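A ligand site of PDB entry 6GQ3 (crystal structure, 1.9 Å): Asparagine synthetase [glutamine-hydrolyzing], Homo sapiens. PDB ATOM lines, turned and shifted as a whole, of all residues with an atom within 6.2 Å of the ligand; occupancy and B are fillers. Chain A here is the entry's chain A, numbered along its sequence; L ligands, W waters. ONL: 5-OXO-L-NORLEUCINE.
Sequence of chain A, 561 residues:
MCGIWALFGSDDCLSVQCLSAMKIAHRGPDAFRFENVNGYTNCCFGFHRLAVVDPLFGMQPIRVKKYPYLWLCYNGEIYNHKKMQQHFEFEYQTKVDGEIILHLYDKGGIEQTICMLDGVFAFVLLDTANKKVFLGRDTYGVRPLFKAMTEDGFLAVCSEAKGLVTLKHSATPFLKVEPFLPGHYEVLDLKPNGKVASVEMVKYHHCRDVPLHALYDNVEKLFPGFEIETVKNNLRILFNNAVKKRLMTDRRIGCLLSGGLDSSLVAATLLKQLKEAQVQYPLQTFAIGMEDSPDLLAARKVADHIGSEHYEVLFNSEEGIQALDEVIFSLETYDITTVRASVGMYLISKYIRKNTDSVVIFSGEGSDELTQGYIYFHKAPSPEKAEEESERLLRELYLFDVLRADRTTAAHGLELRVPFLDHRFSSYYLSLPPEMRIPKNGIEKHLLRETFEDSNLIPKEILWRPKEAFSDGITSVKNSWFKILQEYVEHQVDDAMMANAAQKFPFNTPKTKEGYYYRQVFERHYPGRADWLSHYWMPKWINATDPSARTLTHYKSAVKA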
ATOM      1  N   CYS A   2       3.119 -27.565  -1.868  1.00  0.00           N
ATOM      2  CA  CYS A   2       4.429 -28.135  -2.287  1.00  0.00           C
ATOM      3  C   CYS A   2       4.826 -29.212  -1.294  1.00  0.00           C
ATOM      4  O   CYS A   2       4.503 -29.118  -0.105  1.00  0.00           O
ATOM      5  CB  CYS A   2       5.533 -27.060  -2.343  1.00  0.00           C
ATOM      6  SG  CYS A   2       5.266 -25.832  -3.643  1.00  0.00           S
ATOM      7  N   GLY A   3       5.534 -30.205  -1.796  1.00  0.00           N
ATOM      8  CA  GLY A   3       6.047 -31.318  -1.004  1.00  0.00           C
ATOM      9  C   GLY A   3       7.539 -31.406  -1.114  1.00  0.00           C
ATOM     10  O   GLY A   3       8.087 -31.494  -2.237  1.00  0.00           O
ATOM     11  N   ARG A  27       0.783 -32.977  -2.937  1.00  0.00           N
ATOM     12  CA  ARG A  27       1.012 -31.594  -2.457  1.00  0.00           C
ATOM     13  C   ARG A  27       1.391 -30.625  -3.556  1.00  0.00           C
ATOM     14  O   ARG A  27       1.074 -29.449  -3.442  1.00  0.00           O
ATOM     15  CB  ARG A  27       2.068 -31.544  -1.363  1.00  0.00           C
ATOM     16  CG  ARG A  27       1.827 -32.385  -0.117  1.00  0.00           C
ATOM     17  CD  ARG A  27       2.891 -32.121   0.960  1.00  0.00           C
ATOM     18  NE  ARG A  27       2.842 -30.776   1.520  1.00  0.00           N
ATOM     19  CZ  ARG A  27       2.057 -30.354   2.514  1.00  0.00           C
ATOM     20  NH1 ARG A  27       1.257 -31.177   3.172  1.00  0.00           N
ATOM     21  NH2 ARG A  27       2.105 -29.096   2.911  1.00  0.00           N
ATOM     22  N   GLY A  28       2.073 -31.104  -4.612  1.00  0.00           N
ATOM     23  CA  GLY A  28       2.618 -30.213  -5.666  1.00  0.00           C
ATOM     24  C   GLY A  28       2.407 -30.790  -7.045  1.00  0.00           C
ATOM     25  O   GLY A  28       3.317 -31.376  -7.615  1.00  0.00           O
ATOM     26  N   PHE A  47      11.290 -32.637  -4.999  1.00  0.00           N
ATOM     27  CA  PHE A  47      10.428 -31.502  -4.804  1.00  0.00           C
ATOM     28  C   PHE A  47       9.246 -31.563  -5.740  1.00  0.00           C
ATOM     29  O   PHE A  47       9.440 -31.627  -6.950  1.00  0.00           O
ATOM     30  CB  PHE A  47      11.174 -30.184  -5.077  1.00  0.00           C
ATOM     31  CG  PHE A  47      10.339 -28.976  -4.791  1.00  0.00           C
ATOM     32  CD1 PHE A  47       9.988 -28.665  -3.487  1.00  0.00           C
ATOM     33  CD2 PHE A  47       9.850 -28.169  -5.841  1.00  0.00           C
ATOM     34  CE1 PHE A  47       9.173 -27.568  -3.202  1.00  0.00           C
ATOM     35  CE2 PHE A  47       9.054 -27.075  -5.544  1.00  0.00           C
ATOM     36  CZ  PHE A  47       8.703 -26.782  -4.229  1.00  0.00           C
ATOM     37  N   HIS A  48       8.036 -31.591  -5.169  1.00  0.00           N
ATOM     38  CA  HIS A  48       6.805 -31.513  -5.939  1.00  0.00           C
ATOM     39  C   HIS A  48       6.260 -30.103  -5.791  1.00  0.00           C
ATOM     40  O   HIS A  48       5.949 -29.670  -4.685  1.00  0.00           O
ATOM     41  CB  HIS A  48       5.797 -32.519  -5.428  1.00  0.00           C
ATOM     42  CG  HIS A  48       6.235 -33.943  -5.575  1.00  0.00           C
ATOM     43  ND1 HIS A  48       6.002 -34.673  -6.733  1.00  0.00           N
ATOM     44  CD2 HIS A  48       6.891 -34.770  -4.736  1.00  0.00           C
ATOM     45  CE1 HIS A  48       6.521 -35.885  -6.585  1.00  0.00           C
ATOM     46  NE2 HIS A  48       7.056 -35.971  -5.376  1.00  0.00           N
ATOM     47  N   ARG A  49       6.133 -29.393  -6.906  1.00  0.00           N
ATOM     48  CA  ARG A  49       5.744 -28.012  -6.865  1.00  0.00           C
ATOM     49  C   ARG A  49       4.263 -27.771  -7.163  1.00  0.00           C
ATOM     50  O   ARG A  49       3.727 -28.293  -8.139  1.00  0.00           O
ATOM     51  CB  ARG A  49       6.572 -27.209  -7.882  1.00  0.00           C
ATOM     52  CG  ARG A  49       6.382 -25.719  -7.650  1.00  0.00           C
ATOM     53  CD  ARG A  49       7.346 -24.865  -8.420  1.00  0.00           C
ATOM     54  NE  ARG A  49       7.138 -23.471  -8.103  1.00  0.00           N
ATOM     55  CZ  ARG A  49       7.336 -22.445  -8.921  1.00  0.00           C
ATOM     56  NH1 ARG A  49       7.757 -22.629 -10.176  1.00  0.00           N
ATOM     57  NH2 ARG A  49       7.078 -21.225  -8.485  1.00  0.00           N
ATOM     58  N   LEU A  50       3.616 -26.990  -6.301  1.00  0.00           N
ATOM     59  CA  LEU A  50       2.439 -26.224  -6.676  1.00  0.00           C
ATOM     60  C   LEU A  50       2.960 -24.801  -6.929  1.00  0.00           C
ATOM     61  O   LEU A  50       3.448 -24.150  -6.006  1.00  0.00           O
ATOM     62  CB  LEU A  50       1.416 -26.223  -5.566  1.00  0.00           C
ATOM     63  CG  LEU A  50       0.127 -25.408  -5.780  1.00  0.00           C
ATOM     64  CD1 LEU A  50      -0.733 -26.053  -6.861  1.00  0.00           C
ATOM     65  CD2 LEU A  50      -0.642 -25.332  -4.469  1.00  0.00           C
ATOM     66  N   ALA A  51       2.880 -24.324  -8.160  1.00  0.00           N
ATOM     67  CA  ALA A  51       3.509 -23.029  -8.498  1.00  0.00           C
ATOM     68  C   ALA A  51       2.571 -21.851  -8.178  1.00  0.00           C
ATOM     69  O   ALA A  51       1.637 -21.587  -8.935  1.00  0.00           O
ATOM     70  CB  ALA A  51       3.934 -23.032  -9.962  1.00  0.00           C
ATOM     71  N   VAL A  52       2.879 -21.142  -7.084  1.00  0.00           N
ATOM     72  CA  VAL A  52       2.026 -20.110  -6.519  1.00  0.00           C
ATOM     73  C   VAL A  52       2.585 -18.721  -6.846  1.00  0.00           C
ATOM     74  O   VAL A  52       1.833 -17.852  -7.197  1.00  0.00           O
ATOM     75  CB  VAL A  52       1.820 -20.332  -4.997  1.00  0.00           C
ATOM     76  CG1 VAL A  52       0.893 -19.294  -4.394  1.00  0.00           C
ATOM     77  CG2 VAL A  52       1.183 -21.702  -4.738  1.00  0.00           C
ATOM     78  N   VAL A  53       3.911 -18.545  -6.735  1.00  0.00           N
ATOM     79  CA  VAL A  53       4.614 -17.297  -7.051  1.00  0.00           C
ATOM     80  C   VAL A  53       5.690 -17.712  -8.050  1.00  0.00           C
ATOM     81  O   VAL A  53       6.375 -18.701  -7.823  1.00  0.00           O
ATOM     82  CB  VAL A  53       5.277 -16.724  -5.787  1.00  0.00           C
ATOM     83  CG1 VAL A  53       6.054 -15.443  -6.105  1.00  0.00           C
ATOM     84  CG2 VAL A  53       4.232 -16.479  -4.699  1.00  0.00           C
ATOM     85  N   ASP A  54       5.788 -16.999  -9.173  1.00  0.00           N
ATOM     86  CA  ASP A  54       6.890 -17.187 -10.154  1.00  0.00           C
ATOM     87  C   ASP A  54       6.836 -18.526 -10.886  1.00  0.00           C
ATOM     88  O   ASP A  54       7.696 -19.406 -10.670  1.00  0.00           O
ATOM     89  CB  ASP A  54       8.263 -16.965  -9.494  1.00  0.00           C
ATOM     90  CG  ASP A  54       9.436 -17.091 -10.500  1.00  0.00           C
ATOM     91  OD1 ASP A  54       9.211 -17.103 -11.738  1.00  0.00           O
ATOM     92  OD2 ASP A  54      10.590 -17.172 -10.028  1.00  0.00           O
ATOM     93  N   GLY A  58      10.801 -20.409 -10.593  1.00  0.00           N
ATOM     94  CA  GLY A  58      10.796 -20.799  -9.183  1.00  0.00           C
ATOM     95  C   GLY A  58      10.931 -22.266  -8.857  1.00  0.00           C
ATOM     96  O   GLY A  58      10.702 -22.645  -7.706  1.00  0.00           O
ATOM     97  N   GLN A  60      12.416 -25.798  -7.663  1.00  0.00           N
ATOM     98  CA  GLN A  60      13.363 -26.066  -6.565  1.00  0.00           C
ATOM     99  C   GLN A  60      13.980 -27.450  -6.810  1.00  0.00           C
ATOM    100  O   GLN A  60      13.386 -28.185  -7.600  1.00  0.00           O
ATOM    101  CB  GLN A  60      12.653 -26.031  -5.221  1.00  0.00           C
ATOM    102  CG  GLN A  60      11.736 -24.843  -4.988  1.00  0.00           C
ATOM    103  CD  GLN A  60      11.344 -24.671  -3.534  1.00  0.00           C
ATOM    104  OE1 GLN A  60      12.041 -25.150  -2.628  1.00  0.00           O
ATOM    105  NE2 GLN A  60      10.222 -23.982  -3.280  1.00  0.00           N
ATOM    106  N   TYR A  74      11.955 -25.668   0.024  1.00  0.00           N
ATOM    107  CA  TYR A  74      10.991 -25.214   1.055  1.00  0.00           C
ATOM    108  C   TYR A  74       9.563 -25.316   0.565  1.00  0.00           C
ATOM    109  O   TYR A  74       9.275 -25.148  -0.644  1.00  0.00           O
ATOM    110  CB  TYR A  74      11.336 -23.801   1.576  1.00  0.00           C
ATOM    111  CG  TYR A  74      10.777 -22.666   0.778  1.00  0.00           C
ATOM    112  CD1 TYR A  74      11.116 -22.485  -0.544  1.00  0.00           C
ATOM    113  CD2 TYR A  74       9.821 -21.796   1.341  1.00  0.00           C
ATOM    114  CE1 TYR A  74      10.565 -21.470  -1.299  1.00  0.00           C
ATOM    115  CE2 TYR A  74       9.279 -20.791   0.605  1.00  0.00           C
ATOM    116  CZ  TYR A  74       9.635 -20.635  -0.716  1.00  0.00           C
ATOM    117  OH  TYR A  74       9.061 -19.617  -1.431  1.00  0.00           O
ATOM    118  N   ASN A  75       8.684 -25.550   1.517  1.00  0.00           N
ATOM    119  CA  ASN A  75       7.235 -25.401   1.282  1.00  0.00           C
ATOM    120  C   ASN A  75       6.778 -24.235   2.109  1.00  0.00           C
ATOM    121  O   ASN A  75       6.757 -24.309   3.335  1.00  0.00           O
ATOM    122  CB  ASN A  75       6.572 -26.716   1.693  1.00  0.00           C
ATOM    123  CG  ASN A  75       5.061 -26.676   1.803  1.00  0.00           C
ATOM    124  OD1 ASN A  75       4.512 -27.446   2.593  1.00  0.00           O
ATOM    125  ND2 ASN A  75       4.376 -25.871   0.971  1.00  0.00           N
ATOM    126  N   GLY A  76       6.326 -23.176   1.456  1.00  0.00           N
ATOM    127  CA  GLY A  76       5.947 -21.977   2.231  1.00  0.00           C
ATOM    128  C   GLY A  76       5.774 -20.702   1.435  1.00  0.00           C
ATOM    129  O   GLY A  76       5.916 -20.700   0.224  1.00  0.00           O
ATOM    130  N   GLU A  77       5.509 -19.626   2.167  1.00  0.00           N
ATOM    131  CA  GLU A  77       5.326 -18.311   1.632  1.00  0.00           C
ATOM    132  C   GLU A  77       5.957 -17.288   2.553  1.00  0.00           C
ATOM    133  O   GLU A  77       5.541 -17.157   3.696  1.00  0.00           O
ATOM    134  CB  GLU A  77       3.838 -18.001   1.472  1.00  0.00           C
ATOM    135  CG  GLU A  77       3.051 -18.911   0.537  1.00  0.00           C
ATOM    136  CD  GLU A  77       3.502 -18.839  -0.934  1.00  0.00           C
ATOM    137  OE1 GLU A  77       3.062 -19.654  -1.768  1.00  0.00           O
ATOM    138  OE2 GLU A  77       4.284 -17.947  -1.302  1.00  0.00           O
ATOM    139  N   ILE A  78       6.956 -16.570   2.062  1.00  0.00           N
ATOM    140  CA  ILE A  78       7.659 -15.518   2.849  1.00  0.00           C
ATOM    141  C   ILE A  78       7.051 -14.202   2.398  1.00  0.00           C
ATOM    142  O   ILE A  78       7.494 -13.609   1.403  1.00  0.00           O
ATOM    143  CB  ILE A  78       9.180 -15.526   2.586  1.00  0.00           C
ATOM    144  CG1 ILE A  78       9.758 -16.965   2.670  1.00  0.00           C
ATOM    145  CG2 ILE A  78       9.875 -14.582   3.572  1.00  0.00           C
ATOM    146  CD1 ILE A  78       9.385 -17.704   3.945  1.00  0.00           C
ATOM    147  N   VAL A  96      10.975 -15.781  -7.064  1.00  0.00           N
ATOM    148  CA  VAL A  96      10.246 -16.536  -6.043  1.00  0.00           C
ATOM    149  C   VAL A  96      10.583 -15.999  -4.641  1.00  0.00           C
ATOM    150  O   VAL A  96      11.721 -15.667  -4.353  1.00  0.00           O
ATOM    151  CB  VAL A  96      10.466 -18.063  -6.210  1.00  0.00           C
ATOM    152  CG1 VAL A  96      11.794 -18.534  -5.613  1.00  0.00           C
ATOM    153  CG2 VAL A  96       9.294 -18.834  -5.625  1.00  0.00           C
ATOM    154  N   ASP A  97       9.557 -15.879  -3.808  1.00  0.00           N
ATOM    155  CA  ASP A  97       9.703 -15.373  -2.445  1.00  0.00           C
ATOM    156  C   ASP A  97      10.782 -16.065  -1.641  1.00  0.00           C
ATOM    157  O   ASP A  97      11.512 -15.395  -0.895  1.00  0.00           O
ATOM    158  CB  ASP A  97       8.361 -15.428  -1.698  1.00  0.00           C
ATOM    159  CG  ASP A  97       7.781 -16.810  -1.648  1.00  0.00           C
ATOM    160  OD1 ASP A  97       7.322 -17.292  -2.700  1.00  0.00           O
ATOM    161  OD2 ASP A  97       7.808 -17.423  -0.549  1.00  0.00           O
ATOM    162  N   GLY A  98      10.924 -17.395  -1.756  1.00  0.00           N
ATOM    163  CA  GLY A  98      11.913 -18.088  -0.914  1.00  0.00           C
ATOM    164  C   GLY A  98      13.400 -17.796  -1.192  1.00  0.00           C
ATOM    165  O   GLY A  98      14.270 -18.102  -0.356  1.00  0.00           O
ATOM    166  N   ARG A 143       3.121 -24.928   7.998  1.00  0.00           N
ATOM    167  CA  ARG A 143       3.641 -25.811   6.969  1.00  0.00           C
ATOM    168  C   ARG A 143       4.368 -26.976   7.677  1.00  0.00           C
ATOM    169  O   ARG A 143       5.089 -26.737   8.637  1.00  0.00           O
ATOM    170  CB  ARG A 143       4.587 -25.055   6.042  1.00  0.00           C
ATOM    171  CG  ARG A 143       3.864 -24.020   5.211  1.00  0.00           C
ATOM    172  CD  ARG A 143       2.899 -24.629   4.177  1.00  0.00           C
ATOM    173  NE  ARG A 143       2.425 -23.578   3.273  1.00  0.00           N
ATOM    174  CZ  ARG A 143       1.288 -22.902   3.380  1.00  0.00           C
ATOM    175  NH1 ARG A 143       1.027 -21.934   2.501  1.00  0.00           N
ATOM    176  NH2 ARG A 143       0.421 -23.142   4.372  1.00  0.00           N
ATOM    177  N   MET A 248      -0.159 -12.336  -2.000  1.00  0.00           N
ATOM    178  CA  MET A 248       1.061 -12.598  -2.820  1.00  0.00           C
ATOM    179  C   MET A 248       0.947 -13.948  -3.523  1.00  0.00           C
ATOM    180  O   MET A 248       1.125 -14.985  -2.913  1.00  0.00           O
ATOM    181  CB  MET A 248       2.309 -12.597  -1.940  1.00  0.00           C
ATOM    182  CG  MET A 248       3.664 -12.829  -2.634  1.00  0.00           C
ATOM    183  SD  MET A 248       5.000 -12.954  -1.402  1.00  0.00           S
ATOM    184  CE  MET A 248       4.702 -14.654  -0.851  1.00  0.00           C
ATOM    185  N   GLU A 415      -3.221 -24.701  -1.767  1.00  0.00           N
ATOM    186  CA  GLU A 415      -2.374 -24.062  -0.738  1.00  0.00           C
ATOM    187  C   GLU A 415      -3.218 -23.302   0.294  1.00  0.00           C
ATOM    188  O   GLU A 415      -3.850 -22.303  -0.029  1.00  0.00           O
ATOM    189  CB  GLU A 415      -1.363 -23.075  -1.348  1.00  0.00           C
ATOM    190  CG  GLU A 415      -0.509 -22.398  -0.275  1.00  0.00           C
ATOM    191  CD  GLU A 415       0.369 -21.299  -0.807  1.00  0.00           C
ATOM    192  OE1 GLU A 415      -0.184 -20.226  -1.076  1.00  0.00           O
ATOM    193  OE2 GLU A 415       1.598 -21.532  -0.942  1.00  0.00           O
ATOM    194  N   ARG A 417      -3.955 -20.736   3.364  1.00  0.00           N
ATOM    195  CA  ARG A 417      -3.496 -19.506   4.026  1.00  0.00           C
ATOM    196  C   ARG A 417      -4.406 -19.178   5.190  1.00  0.00           C
ATOM    197  O   ARG A 417      -5.623 -19.311   5.065  1.00  0.00           O
ATOM    198  CB  ARG A 417      -3.378 -18.344   3.032  1.00  0.00           C
ATOM    199  CG  ARG A 417      -2.319 -18.633   2.009  1.00  0.00           C
ATOM    200  CD  ARG A 417      -1.951 -17.475   1.123  1.00  0.00           C
ATOM    201  NE  ARG A 417      -0.960 -17.879   0.121  1.00  0.00           N
ATOM    202  CZ  ARG A 417      -0.318 -17.041  -0.684  1.00  0.00           C
ATOM    203  NH1 ARG A 417      -0.578 -15.741  -0.670  1.00  0.00           N
ATOM    204  NH2 ARG A 417       0.594 -17.509  -1.522  1.00  0.00           N
HETATM  205  N   ONL L   1       6.087 -19.770  -2.633  1.00  0.00           N
HETATM  206  CA  ONL L   1       6.771 -20.822  -3.434  1.00  0.00           C
HETATM  207  C   ONL L   1       6.226 -20.881  -4.817  1.00  0.00           C
HETATM  208  O   ONL L   1       5.140 -20.320  -5.035  1.00  0.00           O
HETATM  209  OXT ONL L   1       6.836 -21.520  -5.703  1.00  0.00           O
HETATM  210  CB  ONL L   1       6.589 -22.205  -2.819  1.00  0.00           C
HETATM  211  CG  ONL L   1       5.085 -22.576  -2.820  1.00  0.00           C
HETATM  212  CD  ONL L   1       4.881 -23.867  -2.082  1.00  0.00           C
HETATM  213  OD  ONL L   1       5.347 -24.027  -0.971  1.00  0.00           O
HETATM  214  CE  ONL L   1       4.149 -24.964  -2.812  1.00  0.00           C
HETATM  215  O   HOH W   1       9.001 -22.939  -5.576  1.00  0.00           O
HETATM  216  O   HOH W   2       2.950 -23.121   0.516  1.00  0.00           O
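Water W1 lies within hydrogen-bond range of an oxygen (OXT) of the ligand (2.6 Å), the backbone carbonyl oxygen of Gly 58 (2.7 Å), the side-chain amide nitrogen of Gln 60 (2.8 Å) and the guanidinium group of Arg 49 (3.2 Å). Water W2 lies within hydrogen-bond range of OE2 of Glu 415 (2.5 Å), NE of Arg 143 (2.8 Å), OD of the ligand (3.0 Å) and ND2 of Asn 75 (3.1 Å).
N of Gly 76 sits at hydrogen-bond distance from OD of the ligand. OD1 of Asp 97 is in salt-bridge range of N of the ligand (2.8 Å). N of the ligand is in salt-bridge range of OE2 of Glu 77 (2.9 Å). SG of Cys 2 is bonded to CE of the ligand (1.6 Å). A nitrogen (N) of the ligand sits at hydrogen-bond distance from the backbone carbonyl oxygen (O) of Gly 76 (3.0 Å). OXT of the ligand is in salt-bridge range of NH2 of Arg 49, 2.8 Å away. O of the ligand is in hydrogen-bond range of N of Val 53 (2.7 Å). OH of Tyr 74 lies within hydrogen-bond range of N of the ligand (3.2 Å). The backbone NH (N) of Val 52 sits at hydrogen-bond distance from an oxygen (O) of the ligand (3.2 Å). OD of the ligand is in hydrogen-bond range of ND2 of Asn 75 (2.8 Å).
The backbone NH (N) of Val 96 is in hydrogen-bond range of the side-chain carboxylate (OD2) of Asp 54 (3.3 Å). The side-chain carboxylate (OD2) of Asp 97 sits at hydrogen-bond distance from the backbone NH (N) of Ile 78, 2.9 Å away. The side-chain carboxylate of Asp 97 sits at hydrogen-bond distance from the side-chain hydroxyl of Tyr 74. The backbone NH (N) of Leu 50 sits at hydrogen-bond distance from the side-chain sulfur (SG) of Cys 2, at 3.3 Å. The side-chain carboxylate of Glu 77 lies close to the side-chain carboxylate of Glu 415. O of Asp 54 lies within hydrogen-bond range of NH2 of Arg 49 (2.9 Å). The guanidinium group of Arg 417 is in salt-bridge range of the side-chain carboxylate of Glu 77 (3.3 Å). The guanidinium group (NE) of Arg 27 sits at hydrogen-bond distance from the backbone carbonyl oxygen (O) of Cys 2 (2.9 Å).
Merely in contact with the ligand: Leu 50 and Val 96. Hydrophobic or aromatic side chains within 4 Å of the ligand: Val 52, Val 53, Tyr 74 and Val 96.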
